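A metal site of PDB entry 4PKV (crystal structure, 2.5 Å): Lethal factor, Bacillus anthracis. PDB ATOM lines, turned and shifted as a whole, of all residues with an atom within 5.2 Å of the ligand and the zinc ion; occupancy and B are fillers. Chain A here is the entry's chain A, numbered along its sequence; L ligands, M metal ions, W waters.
An oxygen (O4) of the ligand is in hydrogen-bond range of the backbone NH (N) of Gly 396 (2.9 Å). A nitrogen (N1) of the ligand is in hydrogen-bond range of the side-chain carboxylate (OE1) of Glu 426 (3.0 Å). The backbone carbonyl oxygen (O) of Gly 396 lies within hydrogen-bond range of a nitrogen (N1) of the ligand. The backbone NH of Lys 395 lies within hydrogen-bond range of an oxygen (O4) of the ligand, at 3.0 Å. The side-chain hydroxyl (OH) of Tyr 467 lies close to an oxygen (O1) of the ligand.
OE1 of Glu 474 lies close to OH of Tyr 467. The side-chain carboxylate (OE2) of Glu 478 lies within salt-bridge range of the guanidinium group (NE) of Arg 481. OE2 of Glu 426 lies close to N of Leu 397 (3.3 Å). OE2 of Glu 426 lies within hydrogen-bond range of N of Tyr 398. OE2 of Glu 478 lies within hydrogen-bond range of ND1 of His 425, 3.0 Å away. O of Gly 396 is in hydrogen-bond range of OG of Ser 394, at 2.7 Å.
OE2 of Glu 478 lies close to F1 of the ligand, at 3.1 Å. The guanidinium group of Arg 481 lies close to a fluorine (F1) of the ligand (3.4 Å). Asp 64 touches the ligand (O to C3, 3.97 Å). Ser 66 touches the ligand (O to C14, 3.5 Å). CB of Asp 67 touches C13 of the ligand, at 3.4 Å. Ser 394 touches the ligand. Val 414 touches the ligand. Leu 416 touches the ligand (CD2 to F1, 3.1 Å). Hydrophobic or aromatic side chains that line the ligand: Val 414, Leu 416, His 425, His 429 and Tyr 467. 15 residues have an atom within 4 Å of the ligand: Asp 64, Ser 66, Asp 67, Ser 394, Lys 395, Gly 396, Val 414, Leu 416, His 425, Glu 426, His 429, Tyr 467, Glu 474, Glu 478 and Arg 481.
Three residues have an atom within 4 Å of the zinc ion: His 425, His 429 and Glu 474.
The zinc ion is bound by an oxygen (O2) of the ligand, an oxygen (O1) of the ligand, a ring nitrogen (NE2) of His 429, the side-chain carboxylate of Glu 474 and a ring nitrogen (NE2) of His 425. The zinc ion has five donor atoms within binding distance.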
ATOM      1  N   ASP A  64      11.908   4.882  10.372  1.00  0.00           N
ATOM      2  CA  ASP A  64      12.881   5.869  10.854  1.00  0.00           C
ATOM      3  C   ASP A  64      13.815   6.324   9.737  1.00  0.00           C
ATOM      4  O   ASP A  64      14.704   7.146   9.950  1.00  0.00           O
ATOM      5  CB  ASP A  64      13.675   5.314  12.032  1.00  0.00           C
ATOM      6  CG  ASP A  64      12.796   5.047  13.257  1.00  0.00           C
ATOM      7  OD1 ASP A  64      12.182   6.004  13.794  1.00  0.00           O
ATOM      8  OD2 ASP A  64      12.726   3.868  13.690  1.00  0.00           O
ATOM      9  N   SER A  66      12.673   7.999   7.310  1.00  0.00           N
ATOM     10  CA  SER A  66      12.021   9.255   6.880  1.00  0.00           C
ATOM     11  C   SER A  66      12.806  10.463   7.309  1.00  0.00           C
ATOM     12  O   SER A  66      13.401  10.482   8.394  1.00  0.00           O
ATOM     13  CB  SER A  66      10.620   9.392   7.462  1.00  0.00           C
ATOM     14  OG  SER A  66       9.974   8.152   7.576  1.00  0.00           O
ATOM     15  N   ASP A  67      12.783  11.502   6.483  1.00  0.00           N
ATOM     16  CA  ASP A  67      13.447  12.734   6.831  1.00  0.00           C
ATOM     17  C   ASP A  67      12.488  13.926   6.869  1.00  0.00           C
ATOM     18  O   ASP A  67      12.899  15.059   6.610  1.00  0.00           O
ATOM     19  CB  ASP A  67      14.602  13.006   5.852  1.00  0.00           C
ATOM     20  CG  ASP A  67      14.178  12.902   4.383  1.00  0.00           C
ATOM     21  OD1 ASP A  67      12.951  12.793   4.115  1.00  0.00           O
ATOM     22  OD2 ASP A  67      15.061  12.973   3.507  1.00  0.00           O
ATOM     23  N   PHE A  68      11.215  13.684   7.197  1.00  0.00           N
ATOM     24  CA  PHE A  68      10.232  14.761   7.188  1.00  0.00           C
ATOM     25  C   PHE A  68       9.113  14.625   8.216  1.00  0.00           C
ATOM     26  O   PHE A  68       8.448  15.611   8.530  1.00  0.00           O
ATOM     27  CB  PHE A  68       9.626  14.903   5.783  1.00  0.00           C
ATOM     28  CG  PHE A  68       9.048  13.632   5.255  1.00  0.00           C
ATOM     29  CD1 PHE A  68       7.747  13.248   5.571  1.00  0.00           C
ATOM     30  CD2 PHE A  68       9.807  12.811   4.413  1.00  0.00           C
ATOM     31  CE1 PHE A  68       7.209  12.057   5.075  1.00  0.00           C
ATOM     32  CE2 PHE A  68       9.286  11.634   3.907  1.00  0.00           C
ATOM     33  CZ  PHE A  68       7.983  11.250   4.241  1.00  0.00           C
ATOM     34  N   VAL A 392       7.777  19.927   5.845  1.00  0.00           N
ATOM     35  CA  VAL A 392       8.786  19.102   6.527  1.00  0.00           C
ATOM     36  C   VAL A 392       8.953  19.449   8.002  1.00  0.00           C
ATOM     37  O   VAL A 392       9.083  20.614   8.347  1.00  0.00           O
ATOM     38  CB  VAL A 392      10.172  19.251   5.791  1.00  0.00           C
ATOM     39  CG1 VAL A 392      11.268  18.420   6.467  1.00  0.00           C
ATOM     40  CG2 VAL A 392      10.043  18.869   4.321  1.00  0.00           C
ATOM     41  N   SER A 394      11.789  18.941  10.780  1.00  0.00           N
ATOM     42  CA  SER A 394      13.164  18.484  10.959  1.00  0.00           C
ATOM     43  C   SER A 394      13.904  19.443  11.878  1.00  0.00           C
ATOM     44  O   SER A 394      13.345  20.455  12.287  1.00  0.00           O
ATOM     45  CB  SER A 394      13.924  18.343   9.612  1.00  0.00           C
ATOM     46  OG  SER A 394      14.128  19.603   8.962  1.00  0.00           O
ATOM     47  N   LYS A 395      15.161  19.129  12.178  1.00  0.00           N
ATOM     48  CA  LYS A 395      16.012  19.994  12.985  1.00  0.00           C
ATOM     49  C   LYS A 395      16.337  21.282  12.222  1.00  0.00           C
ATOM     50  O   LYS A 395      16.471  22.354  12.808  1.00  0.00           O
ATOM     51  CB  LYS A 395      17.310  19.258  13.359  1.00  0.00           C
ATOM     52  CG  LYS A 395      18.332  20.070  14.126  1.00  0.00           C
ATOM     53  CD  LYS A 395      17.954  20.137  15.595  1.00  0.00           C
ATOM     54  CE  LYS A 395      18.968  20.879  16.432  1.00  0.00           C
ATOM     55  NZ  LYS A 395      18.490  20.986  17.840  1.00  0.00           N
ATOM     56  N   GLY A 396      16.482  21.158  10.910  1.00  0.00           N
ATOM     57  CA  GLY A 396      16.957  22.263  10.107  1.00  0.00           C
ATOM     58  C   GLY A 396      16.492  22.167   8.668  1.00  0.00           C
ATOM     59  O   GLY A 396      16.273  21.087   8.135  1.00  0.00           O
ATOM     60  N   LEU A 397      16.325  23.321   8.041  1.00  0.00           N
ATOM     61  CA  LEU A 397      15.816  23.388   6.692  1.00  0.00           C
ATOM     62  C   LEU A 397      16.411  24.605   5.989  1.00  0.00           C
ATOM     63  O   LEU A 397      16.613  25.644   6.596  1.00  0.00           O
ATOM     64  CB  LEU A 397      14.288  23.458   6.711  1.00  0.00           C
ATOM     65  CG  LEU A 397      13.533  23.014   5.447  1.00  0.00           C
ATOM     66  CD1 LEU A 397      13.712  21.527   5.279  1.00  0.00           C
ATOM     67  CD2 LEU A 397      12.054  23.382   5.477  1.00  0.00           C
ATOM     68  N   TYR A 398      16.714  24.477   4.698  1.00  0.00           N
ATOM     69  CA  TYR A 398      16.925  25.663   3.887  1.00  0.00           C
ATOM     70  C   TYR A 398      15.784  25.762   2.862  1.00  0.00           C
ATOM     71  O   TYR A 398      15.503  24.803   2.149  1.00  0.00           O
ATOM     72  CB  TYR A 398      18.288  25.649   3.192  1.00  0.00           C
ATOM     73  CG  TYR A 398      18.473  26.787   2.205  1.00  0.00           C
ATOM     74  CD1 TYR A 398      18.612  28.096   2.651  1.00  0.00           C
ATOM     75  CD2 TYR A 398      18.500  26.567   0.839  1.00  0.00           C
ATOM     76  CE1 TYR A 398      18.755  29.144   1.777  1.00  0.00           C
ATOM     77  CE2 TYR A 398      18.667  27.621  -0.056  1.00  0.00           C
ATOM     78  CZ  TYR A 398      18.789  28.896   0.425  1.00  0.00           C
ATOM     79  OH  TYR A 398      18.948  29.944  -0.442  1.00  0.00           O
ATOM     80  N   GLY A 413      19.000  16.215  16.060  1.00  0.00           N
ATOM     81  CA  GLY A 413      19.248  15.696  14.724  1.00  0.00           C
ATOM     82  C   GLY A 413      19.998  14.381  14.761  1.00  0.00           C
ATOM     83  O   GLY A 413      20.961  14.215  15.514  1.00  0.00           O
ATOM     84  N   VAL A 414      19.538  13.431  13.967  1.00  0.00           N
ATOM     85  CA  VAL A 414      20.246  12.173  13.775  1.00  0.00           C
ATOM     86  C   VAL A 414      21.639  12.448  13.246  1.00  0.00           C
ATOM     87  O   VAL A 414      21.784  13.327  12.394  1.00  0.00           O
ATOM     88  CB  VAL A 414      19.482  11.269  12.788  1.00  0.00           C
ATOM     89  CG1 VAL A 414      20.333  10.065  12.376  1.00  0.00           C
ATOM     90  CG2 VAL A 414      18.119  10.849  13.395  1.00  0.00           C
ATOM     91  N   GLU A 415      22.665  11.753  13.747  1.00  0.00           N
ATOM     92  CA  GLU A 415      23.990  11.854  13.132  1.00  0.00           C
ATOM     93  C   GLU A 415      24.648  13.232  13.406  1.00  0.00           C
ATOM     94  O   GLU A 415      25.688  13.584  12.852  1.00  0.00           O
ATOM     95  CB  GLU A 415      23.846  11.549  11.612  1.00  0.00           C
ATOM     96  CG  GLU A 415      25.007  11.835  10.644  1.00  0.00           C
ATOM     97  CD  GLU A 415      26.052  10.722  10.598  1.00  0.00           C
ATOM     98  OE1 GLU A 415      25.664   9.529  10.687  1.00  0.00           O
ATOM     99  OE2 GLU A 415      27.254  11.040  10.480  1.00  0.00           O
ATOM    100  N   LEU A 416      24.037  14.022  14.291  1.00  0.00           N
ATOM    101  CA  LEU A 416      24.576  15.357  14.597  1.00  0.00           C
ATOM    102  C   LEU A 416      25.169  15.441  16.001  1.00  0.00           C
ATOM    103  O   LEU A 416      24.607  14.911  16.965  1.00  0.00           O
ATOM    104  CB  LEU A 416      23.490  16.414  14.435  1.00  0.00           C
ATOM    105  CG  LEU A 416      23.152  16.829  13.006  1.00  0.00           C
ATOM    106  CD1 LEU A 416      22.147  18.006  13.021  1.00  0.00           C
ATOM    107  CD2 LEU A 416      24.429  17.179  12.216  1.00  0.00           C
ATOM    108  N   GLY A 422      24.386  21.238  12.433  1.00  0.00           N
ATOM    109  CA  GLY A 422      23.143  21.329  11.685  1.00  0.00           C
ATOM    110  C   GLY A 422      23.048  22.615  10.896  1.00  0.00           C
ATOM    111  O   GLY A 422      22.663  22.597   9.716  1.00  0.00           O
ATOM    112  N   HIS A 425      25.351  22.680   7.719  1.00  0.00           N
ATOM    113  CA  HIS A 425      24.815  21.870   6.632  1.00  0.00           C
ATOM    114  C   HIS A 425      23.746  22.685   5.878  1.00  0.00           C
ATOM    115  O   HIS A 425      23.702  22.679   4.637  1.00  0.00           O
ATOM    116  CB  HIS A 425      24.276  20.559   7.204  1.00  0.00           C
ATOM    117  CG  HIS A 425      23.263  19.858   6.349  1.00  0.00           C
ATOM    118  ND1 HIS A 425      23.484  18.624   5.790  1.00  0.00           N
ATOM    119  CD2 HIS A 425      21.993  20.200   6.023  1.00  0.00           C
ATOM    120  CE1 HIS A 425      22.407  18.238   5.117  1.00  0.00           C
ATOM    121  NE2 HIS A 425      21.493  19.179   5.236  1.00  0.00           N
ATOM    122  N   GLU A 426      22.909  23.410   6.613  1.00  0.00           N
ATOM    123  CA  GLU A 426      21.943  24.280   5.970  1.00  0.00           C
ATOM    124  C   GLU A 426      22.637  25.376   5.196  1.00  0.00           C
ATOM    125  O   GLU A 426      22.162  25.806   4.150  1.00  0.00           O
ATOM    126  CB  GLU A 426      20.988  24.926   6.994  1.00  0.00           C
ATOM    127  CG  GLU A 426      20.378  23.950   7.992  1.00  0.00           C
ATOM    128  CD  GLU A 426      19.592  22.842   7.328  1.00  0.00           C
ATOM    129  OE1 GLU A 426      19.496  21.744   7.907  1.00  0.00           O
ATOM    130  OE2 GLU A 426      19.066  23.070   6.205  1.00  0.00           O
ATOM    131  N   HIS A 429      23.368  24.148   1.856  1.00  0.00           N
ATOM    132  CA  HIS A 429      22.338  24.313   0.825  1.00  0.00           C
ATOM    133  C   HIS A 429      22.321  25.711   0.207  1.00  0.00           C
ATOM    134  O   HIS A 429      22.098  25.866  -0.985  1.00  0.00           O
ATOM    135  CB  HIS A 429      20.955  24.032   1.373  1.00  0.00           C
ATOM    136  CG  HIS A 429      20.711  22.600   1.691  1.00  0.00           C
ATOM    137  ND1 HIS A 429      20.908  21.595   0.768  1.00  0.00           N
ATOM    138  CD2 HIS A 429      20.229  22.005   2.807  1.00  0.00           C
ATOM    139  CE1 HIS A 429      20.580  20.436   1.312  1.00  0.00           C
ATOM    140  NE2 HIS A 429      20.167  20.659   2.546  1.00  0.00           N
ATOM    141  N   TYR A 467      23.166   9.501   5.375  1.00  0.00           N
ATOM    142  CA  TYR A 467      22.165  10.444   4.860  1.00  0.00           C
ATOM    143  C   TYR A 467      22.612  11.147   3.550  1.00  0.00           C
ATOM    144  O   TYR A 467      21.771  11.648   2.775  1.00  0.00           O
ATOM    145  CB  TYR A 467      21.821  11.485   5.931  1.00  0.00           C
ATOM    146  CG  TYR A 467      20.756  12.464   5.488  1.00  0.00           C
ATOM    147  CD1 TYR A 467      19.472  12.041   5.150  1.00  0.00           C
ATOM    148  CD2 TYR A 467      21.047  13.819   5.389  1.00  0.00           C
ATOM    149  CE1 TYR A 467      18.510  12.945   4.728  1.00  0.00           C
ATOM    150  CE2 TYR A 467      20.088  14.730   4.973  1.00  0.00           C
ATOM    151  CZ  TYR A 467      18.819  14.293   4.643  1.00  0.00           C
ATOM    152  OH  TYR A 467      17.884  15.234   4.230  1.00  0.00           O
ATOM    153  N   GLU A 474      21.586  16.691  -0.825  1.00  0.00           N
ATOM    154  CA  GLU A 474      21.968  16.275   0.517  1.00  0.00           C
ATOM    155  C   GLU A 474      23.436  15.844   0.551  1.00  0.00           C
ATOM    156  O   GLU A 474      24.159  16.153   1.517  1.00  0.00           O
ATOM    157  CB  GLU A 474      21.060  15.145   1.014  1.00  0.00           C
ATOM    158  CG  GLU A 474      19.566  15.507   1.077  1.00  0.00           C
ATOM    159  CD  GLU A 474      19.303  16.857   1.750  1.00  0.00           C
ATOM    160  OE1 GLU A 474      20.067  17.236   2.644  1.00  0.00           O
ATOM    161  OE2 GLU A 474      18.323  17.536   1.378  1.00  0.00           O
ATOM    162  N   ALA A 477      25.503  18.840   0.749  1.00  0.00           N
ATOM    163  CA  ALA A 477      25.347  19.521   2.023  1.00  0.00           C
ATOM    164  C   ALA A 477      26.145  18.838   3.122  1.00  0.00           C
ATOM    165  O   ALA A 477      26.788  19.501   3.918  1.00  0.00           O
ATOM    166  CB  ALA A 477      23.856  19.609   2.414  1.00  0.00           C
ATOM    167  N   GLU A 478      26.086  17.514   3.146  1.00  0.00           N
ATOM    168  CA  GLU A 478      26.871  16.741   4.112  1.00  0.00           C
ATOM    169  C   GLU A 478      28.385  16.949   3.898  1.00  0.00           C
ATOM    170  O   GLU A 478      29.119  17.300   4.842  1.00  0.00           O
ATOM    171  CB  GLU A 478      26.475  15.267   4.032  1.00  0.00           C
ATOM    172  CG  GLU A 478      25.099  14.960   4.657  1.00  0.00           C
ATOM    173  CD  GLU A 478      25.072  15.107   6.194  1.00  0.00           C
ATOM    174  OE1 GLU A 478      24.975  14.069   6.899  1.00  0.00           O
ATOM    175  OE2 GLU A 478      25.128  16.267   6.697  1.00  0.00           O
ATOM    176  N   ARG A 481      29.440  20.010   5.156  1.00  0.00           N
ATOM    177  CA  ARG A 481      29.442  20.056   6.617  1.00  0.00           C
ATOM    178  C   ARG A 481      30.713  19.416   7.154  1.00  0.00           C
ATOM    179  O   ARG A 481      31.378  19.989   8.014  1.00  0.00           O
ATOM    180  CB  ARG A 481      28.223  19.348   7.214  1.00  0.00           C
ATOM    181  CG  ARG A 481      28.278  19.283   8.732  1.00  0.00           C
ATOM    182  CD  ARG A 481      27.036  18.667   9.330  1.00  0.00           C
ATOM    183  NE  ARG A 481      26.858  17.274   8.955  1.00  0.00           N
ATOM    184  CZ  ARG A 481      27.479  16.254   9.545  1.00  0.00           C
ATOM    185  NH1 ARG A 481      28.347  16.474  10.527  1.00  0.00           N
ATOM    186  NH2 ARG A 481      27.232  15.022   9.129  1.00  0.00           N
HETATM  187  C1  LIG L   1      16.707  17.959   7.254  1.00  0.00           C
HETATM  188  C2  LIG L   1      17.635  18.550   6.191  1.00  0.00           C
HETATM  189  C3  LIG L   1      16.920  10.440  10.091  1.00  0.00           C
HETATM  190  O1  LIG L   1      18.287  17.812   5.106  1.00  0.00           O
HETATM  191  N1  LIG L   1      17.885  19.870   6.186  1.00  0.00           N
HETATM  192  N2  LIG L   1      18.181   9.706   9.773  1.00  0.00           N
HETATM  193  C4  LIG L   1      19.358  17.167   9.612  1.00  0.00           C
HETATM  194  C5  LIG L   1      20.003  15.928   9.645  1.00  0.00           C
HETATM  195  C6  LIG L   1      21.383  15.846   9.537  1.00  0.00           C
HETATM  196  C7  LIG L   1      22.115  17.009   9.372  1.00  0.00           C
HETATM  197  C8  LIG L   1      21.492  18.255   9.318  1.00  0.00           C
HETATM  198  C9  LIG L   1      20.107  18.345   9.438  1.00  0.00           C
HETATM  199  C10 LIG L   1      22.079  14.509   9.579  1.00  0.00           C
HETATM  200  C11 LIG L   1      17.313  15.664   7.523  1.00  0.00           C
HETATM  201  C12 LIG L   1      17.143  14.336   8.238  1.00  0.00           C
HETATM  202  C13 LIG L   1      15.956  13.948   8.878  1.00  0.00           C
HETATM  203  C14 LIG L   1      15.889  12.689   9.488  1.00  0.00           C
HETATM  204  C15 LIG L   1      16.978  11.818   9.442  1.00  0.00           C
HETATM  205  C16 LIG L   1      18.154  12.198   8.783  1.00  0.00           C
HETATM  206  C17 LIG L   1      18.225  13.435   8.180  1.00  0.00           C
HETATM  207  C18 LIG L   1      15.511  17.391   6.482  1.00  0.00           C
HETATM  208  N3  LIG L   1      17.246  16.948   8.223  1.00  0.00           N
HETATM  209  O2  LIG L   1      18.612  20.424   5.190  1.00  0.00           O
HETATM  210  S1  LIG L   1      17.755  17.224   9.704  1.00  0.00           S
HETATM  211  O3  LIG L   1      17.333  16.274  10.738  1.00  0.00           O
HETATM  212  O4  LIG L   1      17.321  18.523  10.181  1.00  0.00           O
HETATM  213  F1  LIG L   1      23.455  16.919   9.276  1.00  0.00           F
HETATM  214 ZN    ZN M   1      19.501  19.035   3.925  1.00  0.00          ZN
HETATM  215  O   HOH W   1      16.988  21.772   3.326  1.00  0.00           O
